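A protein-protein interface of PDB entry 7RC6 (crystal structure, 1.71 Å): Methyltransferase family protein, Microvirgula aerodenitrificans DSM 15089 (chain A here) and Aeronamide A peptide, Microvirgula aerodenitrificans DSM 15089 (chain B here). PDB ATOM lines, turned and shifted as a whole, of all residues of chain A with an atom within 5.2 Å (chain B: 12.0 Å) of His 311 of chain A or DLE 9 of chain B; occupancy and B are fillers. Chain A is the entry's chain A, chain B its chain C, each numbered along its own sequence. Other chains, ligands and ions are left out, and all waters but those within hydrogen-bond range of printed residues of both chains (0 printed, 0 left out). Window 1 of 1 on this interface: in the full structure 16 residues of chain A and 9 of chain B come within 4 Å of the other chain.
A ring nitrogen (NE2) of His 311 of chain A is in hydrogen-bond range of the backbone carbonyl oxygen of Tyr 8 of chain B (3.1 Å).
The indole nitrogen (NE1) of Trp 144 of chain A sits at hydrogen-bond distance from the backbone carbonyl oxygen (O) of Val 36 of chain A (2.9 Å). The backbone NH of Leu 357 of chain A is in hydrogen-bond range of the backbone carbonyl oxygen of His 311 of chain A (2.9 Å). O of Leu 313 of chain A lies within hydrogen-bond range of N of Tyr 355 of chain A (2.8 Å).
Val 36 of chain A touches Tyr 8 of chain B (CG1 to OH, 3.8 Å). Pro 140 of chain A touches DLE 9 of chain B. Trp 144 of chain A touches DLE 9 of chain B (CH2 to CD1, 3.8 Å). CD2 of His 311 of chain A touches O of DLE 9 of chain B, at 3.6 Å. Leu 313 of chain A touches Gly 10 of chain B.
Of chain B, only Tyr 8 and DLE 9 come within 4 Å of His 311 of chain A. Of the printed residues of chain A, DLE 9 of chain B touches Pro 140 (3.6 Å), Trp 144 (3.8 Å) and His 311 (3.6 Å). Of chain B, only Tyr 8 (3.8 Å) comes within 4 Å of Val 36 of chain A. No residue of chain B comes within 4 Å of Thr 37 of chain A. No residue of chain B comes within 4 Å of Ile 309 of chain A. No residue of chain B comes within 4 Å of Asp 310 of chain A. No residue of chain B comes within 4 Å of Val 312 of chain A. Leu 313 of chain A touches just one residue of chain B: Gly 10 (3.7 Å). No residue of chain B comes within 4 Å of Leu 357 of chain A. Of the printed residues of chain B, Trp 144 of chain A touches DLE 9. Printed residues of chain A within 4 Å of Tyr 8 of chain B: Val 36 (3.8 Å) and His 311 (3.1 Å). Printed residues of chain A within 4 Å of Gly 10 of chain B: Leu 313. Ala 12 of chain B touches none of the printed residues of chain A.
Of the 12 printed residues of chain A, 5 touch a printed residue of chain B. Hydrophobic or aromatic side chains of chain A that line the printed part of chain B: Val 36, Pro 140, Trp 144, His 311 and Leu 313. Along chain B the printed residues that touch a printed residue of chain A span positions 8 to 10. Among the printed residues, 6 pairs touch across the chains.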
ATOM      1  N   VAL A  36     -19.714  25.577  -7.362  1.00  0.00           N
ATOM      2  CA  VAL A  36     -19.223  24.618  -8.352  1.00  0.00           C
ATOM      3  C   VAL A  36     -17.731  24.361  -8.178  1.00  0.00           C
ATOM      4  O   VAL A  36     -17.276  23.211  -8.199  1.00  0.00           O
ATOM      5  CB  VAL A  36     -19.543  25.106  -9.773  1.00  0.00           C
ATOM      6  CG1 VAL A  36     -18.920  24.151 -10.801  1.00  0.00           C
ATOM      7  CG2 VAL A  36     -21.084  25.184  -9.953  1.00  0.00           C
ATOM      8  N   THR A  37     -16.940  25.420  -8.015  1.00  0.00           N
ATOM      9  CA  THR A  37     -15.497  25.242  -7.956  1.00  0.00           C
ATOM     10  C   THR A  37     -14.870  26.463  -7.304  1.00  0.00           C
ATOM     11  O   THR A  37     -15.400  27.573  -7.432  1.00  0.00           O
ATOM     12  CB  THR A  37     -14.907  25.026  -9.359  1.00  0.00           C
ATOM     13  OG1 THR A  37     -13.484  24.904  -9.272  1.00  0.00           O
ATOM     14  CG2 THR A  37     -15.244  26.187 -10.278  1.00  0.00           C
ATOM     15  N   PRO A 140     -12.570  21.556  -6.899  1.00  0.00           N
ATOM     16  CA  PRO A 140     -14.006  21.246  -7.014  1.00  0.00           C
ATOM     17  C   PRO A 140     -14.421  20.049  -6.186  1.00  0.00           C
ATOM     18  O   PRO A 140     -15.544  20.031  -5.668  1.00  0.00           O
ATOM     19  CB  PRO A 140     -14.202  20.976  -8.514  1.00  0.00           C
ATOM     20  CG  PRO A 140     -12.806  20.560  -9.007  1.00  0.00           C
ATOM     21  CD  PRO A 140     -11.858  21.415  -8.184  1.00  0.00           C
ATOM     22  N   TRP A 144     -17.720  19.633  -3.782  1.00  0.00           N
ATOM     23  CA  TRP A 144     -18.824  18.701  -3.996  1.00  0.00           C
ATOM     24  C   TRP A 144     -19.029  17.798  -2.791  1.00  0.00           C
ATOM     25  O   TRP A 144     -20.168  17.401  -2.506  1.00  0.00           O
ATOM     26  CB  TRP A 144     -18.611  17.889  -5.276  1.00  0.00           C
ATOM     27  CG  TRP A 144     -18.444  18.754  -6.492  1.00  0.00           C
ATOM     28  CD1 TRP A 144     -18.655  20.108  -6.578  1.00  0.00           C
ATOM     29  CD2 TRP A 144     -18.024  18.333  -7.797  1.00  0.00           C
ATOM     30  NE1 TRP A 144     -18.382  20.553  -7.848  1.00  0.00           N
ATOM     31  CE2 TRP A 144     -17.995  19.483  -8.618  1.00  0.00           C
ATOM     32  CE3 TRP A 144     -17.666  17.093  -8.351  1.00  0.00           C
ATOM     33  CZ2 TRP A 144     -17.619  19.433  -9.959  1.00  0.00           C
ATOM     34  CZ3 TRP A 144     -17.296  17.045  -9.689  1.00  0.00           C
ATOM     35  CH2 TRP A 144     -17.275  18.211 -10.477  1.00  0.00           C
ATOM     36  N   ILE A 309     -21.633  10.447  -8.836  1.00  0.00           N
ATOM     37  CA  ILE A 309     -20.593  10.642  -9.843  1.00  0.00           C
ATOM     38  C   ILE A 309     -20.915  11.916 -10.614  1.00  0.00           C
ATOM     39  O   ILE A 309     -21.871  11.957 -11.393  1.00  0.00           O
ATOM     40  CB  ILE A 309     -20.480   9.427 -10.769  1.00  0.00           C
ATOM     41  CG1 ILE A 309     -20.043   8.206  -9.942  1.00  0.00           C
ATOM     42  CG2 ILE A 309     -19.479   9.712 -11.897  1.00  0.00           C
ATOM     43  CD1 ILE A 309     -19.942   6.913 -10.733  1.00  0.00           C
ATOM     44  N   ASP A 310     -20.117  12.962 -10.404  1.00  0.00           N
ATOM     45  CA  ASP A 310     -20.457  14.264 -10.965  1.00  0.00           C
ATOM     46  C   ASP A 310     -19.598  14.667 -12.154  1.00  0.00           C
ATOM     47  O   ASP A 310     -19.882  15.693 -12.782  1.00  0.00           O
ATOM     48  CB  ASP A 310     -20.376  15.342  -9.878  1.00  0.00           C
ATOM     49  CG  ASP A 310     -21.689  15.511  -9.142  1.00  0.00           C
ATOM     50  OD1 ASP A 310     -22.742  15.559  -9.813  1.00  0.00           O
ATOM     51  OD2 ASP A 310     -21.670  15.574  -7.898  1.00  0.00           O
ATOM     52  N   HIS A 311     -18.556  13.905 -12.477  1.00  0.00           N
ATOM     53  CA  HIS A 311     -17.732  14.211 -13.636  1.00  0.00           C
ATOM     54  C   HIS A 311     -17.007  12.947 -14.070  1.00  0.00           C
ATOM     55  O   HIS A 311     -16.530  12.184 -13.226  1.00  0.00           O
ATOM     56  CB  HIS A 311     -16.720  15.320 -13.323  1.00  0.00           C
ATOM     57  CG  HIS A 311     -16.076  15.904 -14.540  1.00  0.00           C
ATOM     58  ND1 HIS A 311     -16.802  16.460 -15.569  1.00  0.00           N
ATOM     59  CD2 HIS A 311     -14.774  16.016 -14.891  1.00  0.00           C
ATOM     60  CE1 HIS A 311     -15.976  16.893 -16.504  1.00  0.00           C
ATOM     61  NE2 HIS A 311     -14.739  16.637 -16.117  1.00  0.00           N
ATOM     62  N   VAL A 312     -16.933  12.737 -15.386  1.00  0.00           N
ATOM     63  CA  VAL A 312     -16.282  11.571 -15.971  1.00  0.00           C
ATOM     64  C   VAL A 312     -15.276  12.053 -17.006  1.00  0.00           C
ATOM     65  O   VAL A 312     -15.610  12.883 -17.858  1.00  0.00           O
ATOM     66  CB  VAL A 312     -17.299  10.617 -16.625  1.00  0.00           C
ATOM     67  CG1 VAL A 312     -16.604   9.334 -17.077  1.00  0.00           C
ATOM     68  CG2 VAL A 312     -18.442  10.314 -15.667  1.00  0.00           C
ATOM     69  N   LEU A 313     -14.048  11.537 -16.932  1.00  0.00           N
ATOM     70  CA  LEU A 313     -13.018  11.806 -17.929  1.00  0.00           C
ATOM     71  C   LEU A 313     -12.394  10.510 -18.422  1.00  0.00           C
ATOM     72  O   LEU A 313     -12.171   9.584 -17.631  1.00  0.00           O
ATOM     73  CB  LEU A 313     -11.905  12.690 -17.348  1.00  0.00           C
ATOM     74  CG  LEU A 313     -12.197  14.172 -17.148  1.00  0.00           C
ATOM     75  CD1 LEU A 313     -10.994  14.800 -16.470  1.00  0.00           C
ATOM     76  CD2 LEU A 313     -12.474  14.848 -18.480  1.00  0.00           C
ATOM     77  N   TYR A 355     -11.759   8.113 -15.277  1.00  0.00           N
ATOM     78  CA  TYR A 355     -11.701   8.649 -13.919  1.00  0.00           C
ATOM     79  C   TYR A 355     -13.076   9.197 -13.558  1.00  0.00           C
ATOM     80  O   TYR A 355     -13.649   9.990 -14.316  1.00  0.00           O
ATOM     81  CB  TYR A 355     -10.657   9.765 -13.799  1.00  0.00           C
ATOM     82  CG  TYR A 355      -9.205   9.303 -13.791  1.00  0.00           C
ATOM     83  CD1 TYR A 355      -8.628   8.731 -14.921  1.00  0.00           C
ATOM     84  CD2 TYR A 355      -8.413   9.459 -12.658  1.00  0.00           C
ATOM     85  CE1 TYR A 355      -7.303   8.319 -14.924  1.00  0.00           C
ATOM     86  CE2 TYR A 355      -7.080   9.051 -12.645  1.00  0.00           C
ATOM     87  CZ  TYR A 355      -6.530   8.484 -13.778  1.00  0.00           C
ATOM     88  OH  TYR A 355      -5.209   8.084 -13.758  1.00  0.00           O
ATOM     89  N   TYR A 356     -13.592   8.802 -12.391  1.00  0.00           N
ATOM     90  CA  TYR A 356     -14.940   9.165 -11.951  1.00  0.00           C
ATOM     91  C   TYR A 356     -14.846  10.012 -10.688  1.00  0.00           C
ATOM     92  O   TYR A 356     -14.497   9.495  -9.624  1.00  0.00           O
ATOM     93  CB  TYR A 356     -15.777   7.914 -11.675  1.00  0.00           C
ATOM     94  CG  TYR A 356     -16.079   7.064 -12.890  1.00  0.00           C
ATOM     95  CD1 TYR A 356     -17.152   7.364 -13.711  1.00  0.00           C
ATOM     96  CD2 TYR A 356     -15.316   5.939 -13.187  1.00  0.00           C
ATOM     97  CE1 TYR A 356     -17.452   6.581 -14.820  1.00  0.00           C
ATOM     98  CE2 TYR A 356     -15.608   5.148 -14.298  1.00  0.00           C
ATOM     99  CZ  TYR A 356     -16.680   5.478 -15.108  1.00  0.00           C
ATOM    100  OH  TYR A 356     -17.000   4.710 -16.211  1.00  0.00           O
ATOM    101  N   LEU A 357     -15.167  11.303 -10.793  1.00  0.00           N
ATOM    102  CA  LEU A 357     -15.110  12.182  -9.623  1.00  0.00           C
ATOM    103  C   LEU A 357     -16.361  11.925  -8.791  1.00  0.00           C
ATOM    104  O   LEU A 357     -17.467  12.300  -9.191  1.00  0.00           O
ATOM    105  CB  LEU A 357     -15.012  13.651 -10.036  1.00  0.00           C
ATOM    106  CG  LEU A 357     -14.311  14.575  -9.032  1.00  0.00           C
ATOM    107  CD1 LEU A 357     -14.101  15.966  -9.629  1.00  0.00           C
ATOM    108  CD2 LEU A 357     -15.069  14.673  -7.721  1.00  0.00           C
ATOM    109  N   DTH B   7      -9.017  17.912 -19.078  1.00  0.00           N
ATOM    110  CA  DTH B   7      -9.639  19.186 -19.432  1.00  0.00           C
ATOM    111  CB  DTH B   7      -8.652  20.129 -20.159  1.00  0.00           C
ATOM    112  CG2 DTH B   7      -7.456  20.459 -19.266  1.00  0.00           C
ATOM    113  OG1 DTH B   7      -9.324  21.342 -20.524  1.00  0.00           O
ATOM    114  C   DTH B   7     -10.213  19.886 -18.200  1.00  0.00           C
ATOM    115  O   DTH B   7      -9.683  19.757 -17.091  1.00  0.00           O
ATOM    116  N   TYR B   8     -11.294  20.634 -18.405  1.00  0.00           N
ATOM    117  CA  TYR B   8     -12.039  21.222 -17.299  1.00  0.00           C
ATOM    118  C   TYR B   8     -12.587  20.084 -16.446  1.00  0.00           C
ATOM    119  O   TYR B   8     -13.273  19.199 -16.957  1.00  0.00           O
ATOM    120  CB  TYR B   8     -13.168  22.118 -17.823  1.00  0.00           C
ATOM    121  CG  TYR B   8     -14.089  22.681 -16.759  1.00  0.00           C
ATOM    122  CD1 TYR B   8     -13.609  23.534 -15.770  1.00  0.00           C
ATOM    123  CD2 TYR B   8     -15.445  22.372 -16.755  1.00  0.00           C
ATOM    124  CE1 TYR B   8     -14.453  24.057 -14.802  1.00  0.00           C
ATOM    125  CE2 TYR B   8     -16.297  22.888 -15.791  1.00  0.00           C
ATOM    126  CZ  TYR B   8     -15.797  23.730 -14.818  1.00  0.00           C
ATOM    127  OH  TYR B   8     -16.646  24.243 -13.861  1.00  0.00           O
ATOM    128  N   DLE B   9     -12.259  20.088 -15.159  1.00  0.00           N
ATOM    129  CA  DLE B   9     -12.707  19.029 -14.260  1.00  0.00           C
ATOM    130  CB  DLE B   9     -13.333  19.624 -12.992  1.00  0.00           C
ATOM    131  CG  DLE B   9     -14.582  20.478 -13.257  1.00  0.00           C
ATOM    132  CD1 DLE B   9     -15.774  19.616 -13.708  1.00  0.00           C
ATOM    133  CD2 DLE B   9     -14.947  21.339 -12.050  1.00  0.00           C
ATOM    134  C   DLE B   9     -11.589  18.038 -13.915  1.00  0.00           C
ATOM    135  O   DLE B   9     -11.795  17.099 -13.146  1.00  0.00           O
ATOM    136  N   GLY B  10     -10.409  18.240 -14.493  1.00  0.00           N
ATOM    137  CA  GLY B  10      -9.312  17.305 -14.305  1.00  0.00           C
ATOM    138  C   GLY B  10      -8.343  17.666 -13.190  1.00  0.00           C
ATOM    139  O   GLY B  10      -8.313  18.806 -12.724  1.00  0.00           O
ATOM    140  N   DAL B  11      -7.561  16.683 -12.747  1.00  0.00           N
ATOM    141  CA  DAL B  11      -6.480  16.932 -11.786  1.00  0.00           C
ATOM    142  CB  DAL B  11      -5.368  15.883 -11.954  1.00  0.00           C
ATOM    143  C   DAL B  11      -6.866  17.106 -10.290  1.00  0.00           C
ATOM    144  O   DAL B  11      -6.143  17.763  -9.558  1.00  0.00           O
ATOM    145  N   ALA B  12      -7.983  16.532  -9.835  1.00  0.00           N
ATOM    146  CA  ALA B  12      -8.421  16.653  -8.417  1.00  0.00           C
ATOM    147  C   ALA B  12      -7.399  16.064  -7.375  1.00  0.00           C
ATOM    148  O   ALA B  12      -6.748  15.082  -7.740  1.00  0.00           O
ATOM    149  CB  ALA B  12      -9.781  15.980  -8.280  1.00  0.00           C
ATOM    150  N   DSG B  13      -7.245  16.632  -6.134  1.00  0.00           N
ATOM    151  CA  DSG B  13      -6.141  16.230  -5.165  1.00  0.00           C
ATOM    152  C   DSG B  13      -4.838  16.640  -5.848  1.00  0.00           C
ATOM    153  O   DSG B  13      -3.817  16.574  -5.209  1.00  0.00           O
ATOM    154  CB  DSG B  13      -5.888  17.013  -3.763  1.00  0.00           C
ATOM    155  CG  DSG B  13      -6.929  16.784  -2.560  1.00  0.00           C
ATOM    156  OD1 DSG B  13      -8.080  16.428  -2.835  1.00  0.00           O
ATOM    157  ND2 DSG B  13      -6.514  17.163  -1.191  1.00  0.00           N
ATOM    158  N   VAL B  14      -4.857  17.185  -7.064  1.00  0.00           N
ATOM    159  CA  VAL B  14      -3.653  17.815  -7.604  1.00  0.00           C
ATOM    160  C   VAL B  14      -3.876  19.342  -7.737  1.00  0.00           C
ATOM    161  O   VAL B  14      -3.255  20.110  -7.006  1.00  0.00           O
ATOM    162  CB  VAL B  14      -3.225  17.159  -8.948  1.00  0.00           C
ATOM    163  CG1 VAL B  14      -2.474  18.140  -9.844  1.00  0.00           C
ATOM    164  CG2 VAL B  14      -2.390  15.909  -8.686  1.00  0.00           C
ATOM    165  N   DVA B  15      -4.767  19.782  -8.631  1.00  0.00           N
ATOM    166  CA  DVA B  15      -5.017  21.225  -8.804  1.00  0.00           C
ATOM    167  CB  DVA B  15      -6.411  21.509  -9.432  1.00  0.00           C
ATOM    168  CG1 DVA B  15      -6.492  20.947 -10.847  1.00  0.00           C
ATOM    169  CG2 DVA B  15      -7.528  20.941  -8.552  1.00  0.00           C
ATOM    170  C   DVA B  15      -3.895  21.927  -9.582  1.00  0.00           C
ATOM    171  O   DVA B  15      -2.893  21.307  -9.946  1.00  0.00           O
ATOM    172  N   GLY B  16      -4.067  23.226  -9.821  1.00  0.00           N
ATOM    173  CA  GLY B  16      -3.083  24.012 -10.553  1.00  0.00           C
ATOM    174  C   GLY B  16      -2.855  23.518 -11.972  1.00  0.00           C
ATOM    175  O   GLY B  16      -2.323  24.234 -12.821  1.00  0.00           O
